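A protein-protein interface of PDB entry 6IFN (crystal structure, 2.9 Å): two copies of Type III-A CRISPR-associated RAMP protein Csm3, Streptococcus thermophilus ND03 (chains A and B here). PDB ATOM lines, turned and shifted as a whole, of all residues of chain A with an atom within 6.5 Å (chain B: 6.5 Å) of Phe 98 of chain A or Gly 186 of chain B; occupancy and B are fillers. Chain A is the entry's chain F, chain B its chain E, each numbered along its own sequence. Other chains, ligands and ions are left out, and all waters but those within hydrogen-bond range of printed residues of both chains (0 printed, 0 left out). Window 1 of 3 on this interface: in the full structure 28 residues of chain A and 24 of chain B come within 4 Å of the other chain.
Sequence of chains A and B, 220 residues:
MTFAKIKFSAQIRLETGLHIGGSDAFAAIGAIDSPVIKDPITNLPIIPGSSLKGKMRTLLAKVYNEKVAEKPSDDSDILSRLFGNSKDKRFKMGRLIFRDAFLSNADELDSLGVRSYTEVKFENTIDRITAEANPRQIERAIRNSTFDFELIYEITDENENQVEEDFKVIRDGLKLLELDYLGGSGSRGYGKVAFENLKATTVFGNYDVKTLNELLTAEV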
ATOM      1  N   GLY A  49      10.133  21.582  10.327  1.00  0.00           N
ATOM      2  CA  GLY A  49      10.372  22.983  10.608  1.00  0.00           C
ATOM      3  C   GLY A  49       9.077  23.744  10.812  1.00  0.00           C
ATOM      4  O   GLY A  49       9.050  24.748  11.494  1.00  0.00           O
ATOM      5  N   SER A  50       7.994  23.273  10.179  1.00  0.00           N
ATOM      6  CA  SER A  50       6.696  23.912  10.300  1.00  0.00           C
ATOM      7  C   SER A  50       6.287  23.949  11.779  1.00  0.00           C
ATOM      8  O   SER A  50       5.799  24.989  12.264  1.00  0.00           O
ATOM      9  CB  SER A  50       5.677  23.207   9.449  1.00  0.00           C
ATOM     10  OG  SER A  50       5.888  21.806   9.430  1.00  0.00           O
ATOM     11  N   LEU A  52       8.366  23.658  14.538  1.00  0.00           N
ATOM     12  CA  LEU A  52       9.243  24.595  15.293  1.00  0.00           C
ATOM     13  C   LEU A  52       8.754  26.035  15.128  1.00  0.00           C
ATOM     14  O   LEU A  52       8.591  26.760  16.110  1.00  0.00           O
ATOM     15  CB  LEU A  52      10.681  24.524  14.785  1.00  0.00           C
ATOM     16  CG  LEU A  52      11.367  23.172  14.899  1.00  0.00           C
ATOM     17  CD1 LEU A  52      12.427  22.992  13.821  1.00  0.00           C
ATOM     18  CD2 LEU A  52      11.976  23.028  16.275  1.00  0.00           C
ATOM     19  N   LYS A  53       8.567  26.449  13.871  1.00  0.00           N
ATOM     20  CA  LYS A  53       8.202  27.810  13.566  1.00  0.00           C
ATOM     21  C   LYS A  53       6.872  28.118  14.249  1.00  0.00           C
ATOM     22  O   LYS A  53       6.755  29.090  14.951  1.00  0.00           O
ATOM     23  CB  LYS A  53       8.060  28.033  12.061  1.00  0.00           C
ATOM     24  CG  LYS A  53       7.739  29.468  11.673  1.00  0.00           C
ATOM     25  CD  LYS A  53       7.621  29.700  10.196  1.00  0.00           C
ATOM     26  CE  LYS A  53       7.353  31.155   9.889  1.00  0.00           C
ATOM     27  NZ  LYS A  53       7.021  31.378   8.462  1.00  0.00           N
ATOM     28  N   GLY A  54       5.873  27.263  14.024  1.00  0.00           N
ATOM     29  CA  GLY A  54       4.537  27.510  14.551  1.00  0.00           C
ATOM     30  C   GLY A  54       4.571  27.754  16.052  1.00  0.00           C
ATOM     31  O   GLY A  54       4.115  28.798  16.535  1.00  0.00           O
ATOM     32  N   MET A  56       7.099  28.256  18.213  1.00  0.00           N
ATOM     33  CA  MET A  56       7.911  29.385  18.639  1.00  0.00           C
ATOM     34  C   MET A  56       7.152  30.700  18.390  1.00  0.00           C
ATOM     35  O   MET A  56       7.222  31.627  19.188  1.00  0.00           O
ATOM     36  CB  MET A  56       9.253  29.427  17.911  1.00  0.00           C
ATOM     37  CG  MET A  56      10.087  30.645  18.299  1.00  0.00           C
ATOM     38  SD  MET A  56      11.728  30.735  17.571  1.00  0.00           S
ATOM     39  CE  MET A  56      12.281  29.076  17.963  1.00  0.00           C
ATOM     40  N   LEU A  82       9.880  38.847  11.110  1.00  0.00           N
ATOM     41  CA  LEU A  82      10.715  37.674  11.213  1.00  0.00           C
ATOM     42  C   LEU A  82      10.044  36.458  10.571  1.00  0.00           C
ATOM     43  O   LEU A  82      10.699  35.683   9.891  1.00  0.00           O
ATOM     44  CB  LEU A  82      10.997  37.417  12.693  1.00  0.00           C
ATOM     45  CG  LEU A  82      12.083  38.285  13.299  1.00  0.00           C
ATOM     46  CD1 LEU A  82      11.875  38.408  14.794  1.00  0.00           C
ATOM     47  CD2 LEU A  82      13.464  37.721  12.975  1.00  0.00           C
ATOM     48  N   PHE A  83       8.752  36.262  10.839  1.00  0.00           N
ATOM     49  CA  PHE A  83       8.065  35.020  10.482  1.00  0.00           C
ATOM     50  C   PHE A  83       7.243  35.180   9.205  1.00  0.00           C
ATOM     51  O   PHE A  83       6.715  34.192   8.698  1.00  0.00           O
ATOM     52  CB  PHE A  83       7.154  34.577  11.628  1.00  0.00           C
ATOM     53  CG  PHE A  83       7.932  34.165  12.845  1.00  0.00           C
ATOM     54  CD1 PHE A  83       8.441  35.116  13.704  1.00  0.00           C
ATOM     55  CD2 PHE A  83       8.203  32.832  13.094  1.00  0.00           C
ATOM     56  CE1 PHE A  83       9.170  34.734  14.816  1.00  0.00           C
ATOM     57  CE2 PHE A  83       8.924  32.454  14.212  1.00  0.00           C
ATOM     58  CZ  PHE A  83       9.399  33.401  15.073  1.00  0.00           C
ATOM     59  N   LEU A  96      13.418  34.692   8.475  1.00  0.00           N
ATOM     60  CA  LEU A  96      13.798  33.426   9.079  1.00  0.00           C
ATOM     61  C   LEU A  96      13.420  32.265   8.164  1.00  0.00           C
ATOM     62  O   LEU A  96      12.337  32.248   7.606  1.00  0.00           O
ATOM     63  CB  LEU A  96      13.072  33.273  10.413  1.00  0.00           C
ATOM     64  CG  LEU A  96      13.551  34.180  11.539  1.00  0.00           C
ATOM     65  CD1 LEU A  96      12.592  34.099  12.714  1.00  0.00           C
ATOM     66  CD2 LEU A  96      14.968  33.796  11.966  1.00  0.00           C
ATOM     67  N   ILE A  97      14.310  31.277   8.085  1.00  0.00           N
ATOM     68  CA  ILE A  97      14.045  30.028   7.419  1.00  0.00           C
ATOM     69  C   ILE A  97      14.340  28.915   8.420  1.00  0.00           C
ATOM     70  O   ILE A  97      15.508  28.657   8.701  1.00  0.00           O
ATOM     71  CB  ILE A  97      14.923  29.897   6.160  1.00  0.00           C
ATOM     72  CG1 ILE A  97      14.528  30.907   5.086  1.00  0.00           C
ATOM     73  CG2 ILE A  97      14.938  28.475   5.611  1.00  0.00           C
ATOM     74  CD1 ILE A  97      15.585  31.082   4.023  1.00  0.00           C
ATOM     75  N   PHE A  98      13.284  28.265   8.919  1.00  0.00           N
ATOM     76  CA  PHE A  98      13.394  27.063   9.759  1.00  0.00           C
ATOM     77  C   PHE A  98      13.639  25.864   8.842  1.00  0.00           C
ATOM     78  O   PHE A  98      13.246  25.883   7.691  1.00  0.00           O
ATOM     79  CB  PHE A  98      12.143  26.878  10.625  1.00  0.00           C
ATOM     80  CG  PHE A  98      11.958  27.959  11.654  1.00  0.00           C
ATOM     81  CD1 PHE A  98      12.560  27.864  12.896  1.00  0.00           C
ATOM     82  CD2 PHE A  98      11.241  29.104  11.361  1.00  0.00           C
ATOM     83  CE1 PHE A  98      12.449  28.895  13.824  1.00  0.00           C
ATOM     84  CE2 PHE A  98      11.099  30.118  12.299  1.00  0.00           C
ATOM     85  CZ  PHE A  98      11.717  30.022  13.523  1.00  0.00           C
ATOM     86  N   ARG A  99      14.296  24.830   9.362  1.00  0.00           N
ATOM     87  CA  ARG A  99      14.622  23.661   8.562  1.00  0.00           C
ATOM     88  C   ARG A  99      14.152  22.398   9.288  1.00  0.00           C
ATOM     89  O   ARG A  99      14.272  22.318  10.511  1.00  0.00           O
ATOM     90  CB  ARG A  99      16.121  23.641   8.246  1.00  0.00           C
ATOM     91  CG  ARG A  99      16.623  24.943   7.627  1.00  0.00           C
ATOM     92  CD  ARG A  99      17.386  24.761   6.308  1.00  0.00           C
ATOM     93  NE  ARG A  99      16.882  25.601   5.217  1.00  0.00           N
ATOM     94  CZ  ARG A  99      17.586  25.927   4.140  1.00  0.00           C
ATOM     95  NH1 ARG A  99      18.681  25.254   3.855  1.00  0.00           N
ATOM     96  NH2 ARG A  99      17.232  26.949   3.379  1.00  0.00           N
ATOM     97  N   ASP A 100      13.585  21.454   8.520  1.00  0.00           N
ATOM     98  CA  ASP A 100      13.298  20.136   9.016  1.00  0.00           C
ATOM     99  C   ASP A 100      14.564  19.625   9.723  1.00  0.00           C
ATOM    100  O   ASP A 100      15.668  19.673   9.165  1.00  0.00           O
ATOM    101  CB  ASP A 100      12.896  19.166   7.898  1.00  0.00           C
ATOM    102  CG  ASP A 100      11.491  19.340   7.333  1.00  0.00           C
ATOM    103  OD1 ASP A 100      10.719  20.236   7.852  1.00  0.00           O
ATOM    104  OD2 ASP A 100      11.181  18.576   6.348  1.00  0.00           O
ATOM    105  N   PHE A 149      19.710  20.994  14.228  1.00  0.00           N
ATOM    106  CA  PHE A 149      18.855  22.155  14.127  1.00  0.00           C
ATOM    107  C   PHE A 149      19.568  23.251  13.341  1.00  0.00           C
ATOM    108  O   PHE A 149      20.760  23.517  13.582  1.00  0.00           O
ATOM    109  CB  PHE A 149      18.506  22.703  15.505  1.00  0.00           C
ATOM    110  CG  PHE A 149      17.701  23.978  15.473  1.00  0.00           C
ATOM    111  CD1 PHE A 149      16.402  23.991  15.001  1.00  0.00           C
ATOM    112  CD2 PHE A 149      18.237  25.177  15.925  1.00  0.00           C
ATOM    113  CE1 PHE A 149      15.653  25.164  15.003  1.00  0.00           C
ATOM    114  CE2 PHE A 149      17.488  26.349  15.924  1.00  0.00           C
ATOM    115  CZ  PHE A 149      16.192  26.340  15.472  1.00  0.00           C
ATOM    116  N   GLU A 150      18.805  23.888  12.442  1.00  0.00           N
ATOM    117  CA  GLU A 150      19.292  24.899  11.540  1.00  0.00           C
ATOM    118  C   GLU A 150      18.214  25.960  11.361  1.00  0.00           C
ATOM    119  O   GLU A 150      17.093  25.642  11.091  1.00  0.00           O
ATOM    120  CB  GLU A 150      19.632  24.277  10.193  1.00  0.00           C
ATOM    121  CG  GLU A 150      20.433  25.193   9.295  1.00  0.00           C
ATOM    122  CD  GLU A 150      21.119  24.467   8.149  1.00  0.00           C
ATOM    123  OE1 GLU A 150      21.712  23.383   8.422  1.00  0.00           O
ATOM    124  OE2 GLU A 150      21.041  24.960   6.979  1.00  0.00           O
ATOM    125  N   LEU A 151      18.585  27.223  11.537  1.00  0.00           N
ATOM    126  CA  LEU A 151      17.703  28.355  11.296  1.00  0.00           C
ATOM    127  C   LEU A 151      18.506  29.458  10.584  1.00  0.00           C
ATOM    128  O   LEU A 151      19.605  29.761  10.984  1.00  0.00           O
ATOM    129  CB  LEU A 151      17.148  28.806  12.649  1.00  0.00           C
ATOM    130  CG  LEU A 151      16.441  30.160  12.675  1.00  0.00           C
ATOM    131  CD1 LEU A 151      15.122  30.090  11.907  1.00  0.00           C
ATOM    132  CD2 LEU A 151      16.199  30.639  14.107  1.00  0.00           C
ATOM    133  N   ILE A 152      17.956  30.038   9.519  1.00  0.00           N
ATOM    134  CA  ILE A 152      18.678  31.005   8.701  1.00  0.00           C
ATOM    135  C   ILE A 152      18.066  32.392   8.889  1.00  0.00           C
ATOM    136  O   ILE A 152      16.851  32.551   8.785  1.00  0.00           O
ATOM    137  CB  ILE A 152      18.634  30.619   7.220  1.00  0.00           C
ATOM    138  CG1 ILE A 152      19.177  29.208   6.982  1.00  0.00           C
ATOM    139  CG2 ILE A 152      19.328  31.692   6.389  1.00  0.00           C
ATOM    140  CD1 ILE A 152      20.609  29.014   7.418  1.00  0.00           C
ATOM    141  N   LEU A 174      13.728  30.656  21.491  1.00  0.00           N
ATOM    142  CA  LEU A 174      14.324  29.375  21.795  1.00  0.00           C
ATOM    143  C   LEU A 174      14.156  29.060  23.288  1.00  0.00           C
ATOM    144  O   LEU A 174      13.793  27.942  23.643  1.00  0.00           O
ATOM    145  CB  LEU A 174      15.800  29.395  21.396  1.00  0.00           C
ATOM    146  CG  LEU A 174      16.101  29.571  19.912  1.00  0.00           C
ATOM    147  CD1 LEU A 174      17.550  29.987  19.727  1.00  0.00           C
ATOM    148  CD2 LEU A 174      15.856  28.293  19.140  1.00  0.00           C
ATOM    149  N   TYR B 181      16.158  28.277  -0.076  1.00  0.00           N
ATOM    150  CA  TYR B 181      15.420  27.111  -0.520  1.00  0.00           C
ATOM    151  C   TYR B 181      14.934  27.296  -1.956  1.00  0.00           C
ATOM    152  O   TYR B 181      14.817  28.421  -2.436  1.00  0.00           O
ATOM    153  CB  TYR B 181      14.197  26.908   0.362  1.00  0.00           C
ATOM    154  CG  TYR B 181      13.228  28.061   0.384  1.00  0.00           C
ATOM    155  CD1 TYR B 181      13.414  29.121   1.246  1.00  0.00           C
ATOM    156  CD2 TYR B 181      12.097  28.062  -0.405  1.00  0.00           C
ATOM    157  CE1 TYR B 181      12.513  30.164   1.330  1.00  0.00           C
ATOM    158  CE2 TYR B 181      11.189  29.095  -0.343  1.00  0.00           C
ATOM    159  CZ  TYR B 181      11.405  30.152   0.520  1.00  0.00           C
ATOM    160  OH  TYR B 181      10.512  31.174   0.577  1.00  0.00           O
ATOM    161  N   LEU B 182      14.593  26.164  -2.594  1.00  0.00           N
ATOM    162  CA  LEU B 182      13.927  26.119  -3.884  1.00  0.00           C
ATOM    163  C   LEU B 182      12.414  26.150  -3.657  1.00  0.00           C
ATOM    164  O   LEU B 182      11.872  25.362  -2.890  1.00  0.00           O
ATOM    165  CB  LEU B 182      14.358  24.862  -4.631  1.00  0.00           C
ATOM    166  CG  LEU B 182      14.585  24.997  -6.133  1.00  0.00           C
ATOM    167  CD1 LEU B 182      15.115  26.371  -6.496  1.00  0.00           C
ATOM    168  CD2 LEU B 182      15.530  23.910  -6.645  1.00  0.00           C
ATOM    169  N   GLY B 183      11.770  27.102  -4.345  1.00  0.00           N
ATOM    170  CA  GLY B 183      10.442  27.617  -4.009  1.00  0.00           C
ATOM    171  C   GLY B 183       9.487  26.522  -3.575  1.00  0.00           C
ATOM    172  O   GLY B 183       9.211  25.591  -4.297  1.00  0.00           O
ATOM    173  N   GLY B 184       8.974  26.689  -2.363  1.00  0.00           N
ATOM    174  CA  GLY B 184       8.166  25.725  -1.639  1.00  0.00           C
ATOM    175  C   GLY B 184       7.560  26.449  -0.465  1.00  0.00           C
ATOM    176  O   GLY B 184       7.351  27.659  -0.533  1.00  0.00           O
ATOM    177  N   SER B 185       7.283  25.748   0.621  1.00  0.00           N
ATOM    178  CA  SER B 185       6.952  26.479   1.814  1.00  0.00           C
ATOM    179  C   SER B 185       8.230  26.571   2.648  1.00  0.00           C
ATOM    180  O   SER B 185       8.470  25.784   3.540  1.00  0.00           O
ATOM    181  CB  SER B 185       5.768  25.863   2.493  1.00  0.00           C
ATOM    182  OG  SER B 185       4.769  25.625   1.490  1.00  0.00           O
ATOM    183  N   GLY B 186       9.075  27.521   2.265  1.00  0.00           N
ATOM    184  CA  GLY B 186      10.483  27.472   2.600  1.00  0.00           C
ATOM    185  C   GLY B 186      10.751  27.790   4.057  1.00  0.00           C
ATOM    186  O   GLY B 186      11.594  27.155   4.707  1.00  0.00           O
ATOM    187  N   SER B 187      10.027  28.801   4.543  1.00  0.00           N
ATOM    188  CA  SER B 187      10.099  29.303   5.912  1.00  0.00           C
ATOM    189  C   SER B 187       9.815  28.169   6.906  1.00  0.00           C
ATOM    190  O   SER B 187      10.242  28.223   8.045  1.00  0.00           O
ATOM    191  CB  SER B 187       9.097  30.433   6.102  1.00  0.00           C
ATOM    192  N   ARG B 188       9.036  27.169   6.468  1.00  0.00           N
ATOM    193  CA  ARG B 188       8.553  26.111   7.327  1.00  0.00           C
ATOM    194  C   ARG B 188       9.329  24.819   7.050  1.00  0.00           C
ATOM    195  O   ARG B 188       8.852  23.718   7.370  1.00  0.00           O
ATOM    196  CB  ARG B 188       7.040  25.958   7.135  1.00  0.00           C
ATOM    197  CG  ARG B 188       6.239  27.187   7.566  1.00  0.00           C
ATOM    198  CD  ARG B 188       4.748  26.993   7.385  1.00  0.00           C
ATOM    199  NE  ARG B 188       4.398  26.988   5.982  1.00  0.00           N
ATOM    200  CZ  ARG B 188       4.268  28.084   5.258  1.00  0.00           C
ATOM    201  NH1 ARG B 188       4.401  29.278   5.815  1.00  0.00           N
ATOM    202  NH2 ARG B 188       4.021  27.980   3.974  1.00  0.00           N
ATOM    203  N   GLY B 189      10.511  24.947   6.438  1.00  0.00           N
ATOM    204  CA  GLY B 189      11.484  23.867   6.387  1.00  0.00           C
ATOM    205  C   GLY B 189      11.521  23.121   5.059  1.00  0.00           C
ATOM    206  O   GLY B 189      12.134  22.037   5.008  1.00  0.00           O
ATOM    207  N   TYR B 190      10.932  23.667   3.987  1.00  0.00           N
ATOM    208  CA  TYR B 190      10.797  22.853   2.817  1.00  0.00           C
ATOM    209  C   TYR B 190      12.074  22.756   1.960  1.00  0.00           C
ATOM    210  O   TYR B 190      12.605  21.678   1.844  1.00  0.00           O
ATOM    211  CB  TYR B 190       9.596  23.289   1.984  1.00  0.00           C
ATOM    212  CG  TYR B 190       8.294  22.729   2.477  1.00  0.00           C
ATOM    213  CD1 TYR B 190       8.007  22.731   3.820  1.00  0.00           C
ATOM    214  CD2 TYR B 190       7.345  22.213   1.620  1.00  0.00           C
ATOM    215  CE1 TYR B 190       6.798  22.259   4.301  1.00  0.00           C
ATOM    216  CE2 TYR B 190       6.149  21.702   2.083  1.00  0.00           C
ATOM    217  CZ  TYR B 190       5.871  21.728   3.433  1.00  0.00           C
ATOM    218  OH  TYR B 190       4.705  21.271   3.971  1.00  0.00           O
ATOM    219  N   GLY B 191      12.483  23.799   1.254  1.00  0.00           N
ATOM    220  CA  GLY B 191      13.115  23.534  -0.081  1.00  0.00           C
ATOM    221  C   GLY B 191      14.618  23.321  -0.033  1.00  0.00           C
ATOM    222  O   GLY B 191      15.278  23.614  -0.992  1.00  0.00           O
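Of the 18 printed residues of chain A, 7 touch a printed residue of chain B.
Of the 11 printed residues of chain B, 5 touch a printed residue of chain A.
Among the printed residues, no Asp or Glu carboxylate lies within 4 Å of a Lys or Arg side-chain nitrogen of the other chain.
O of Ile 152 of chain A sits at hydrogen-bond distance from N of Ile 97 of chain A (2.9 Å).
The backbone carbonyl oxygen (O) of Phe 83 of chain A lies within hydrogen-bond range of the side-chain amino group (NZ) of Lys 53 of chain A (2.8 Å).
NH1 of Arg 99 of chain A is in salt-bridge range of OE2 of Glu 150 of chain A.
OD1 of Asp 100 of chain A sits at hydrogen-bond distance from N of Gly 49 of chain A (2.9 Å).
N of Ser 50 of chain A lies within hydrogen-bond range of O of Arg 188 of chain B (3.0 Å).
The backbone NH (N) of Gly 189 of chain B sits close to the backbone carbonyl oxygen (O) of Phe 98 of chain A.
O of Ser 187 of chain B lies within hydrogen-bond range of N of Phe 98 of chain A (3.2 Å).
Of the printed residues of chain B, Phe 98 of chain A touches Gly 186 (3.6 Å), Ser 187 (3.2 Å) and Gly 189 (3.0 Å).
Of chain A, only Ile 97 and Phe 98 come within 4 Å of Gly 186 of chain B.
Printed residues of chain B within 4 Å of Ile 97 of chain A: Gly 186.
Of the printed residues of chain B, Gly 49 of chain A touches Arg 188 (3.4 Å).
Gly 191 of chain B touches none of the printed residues of chain A.
Ile 152 of chain A touches none of the printed residues of chain B.
The nearest residue of chain B that does not touch Phe 98 of chain A is Arg 188 of chain B (4.1 Å).
The nearest printed residue of chain B that does not touch Ile 97 of chain A is Tyr 181 of chain B (4.03 Å).
Among the printed residues, merely in contact across the chains: Lys 53 of chain A with Ser 187 of chain B, Gly 49 of chain A with Arg 188 of chain B, Asp 100 of chain A with Gly 189 of chain B, Phe 98 of chain A with Gly 186 of chain B, Ile 97 of chain A with Gly 186 of chain B, Arg 99 of chain A with Gly 189 of chain B, Arg 99 of chain A with Tyr 181 of chain B, Lys 53 of chain A with Arg 188 of chain B and Asp 100 of chain A with Arg 188 of chain B.
No position is printed for both chains.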
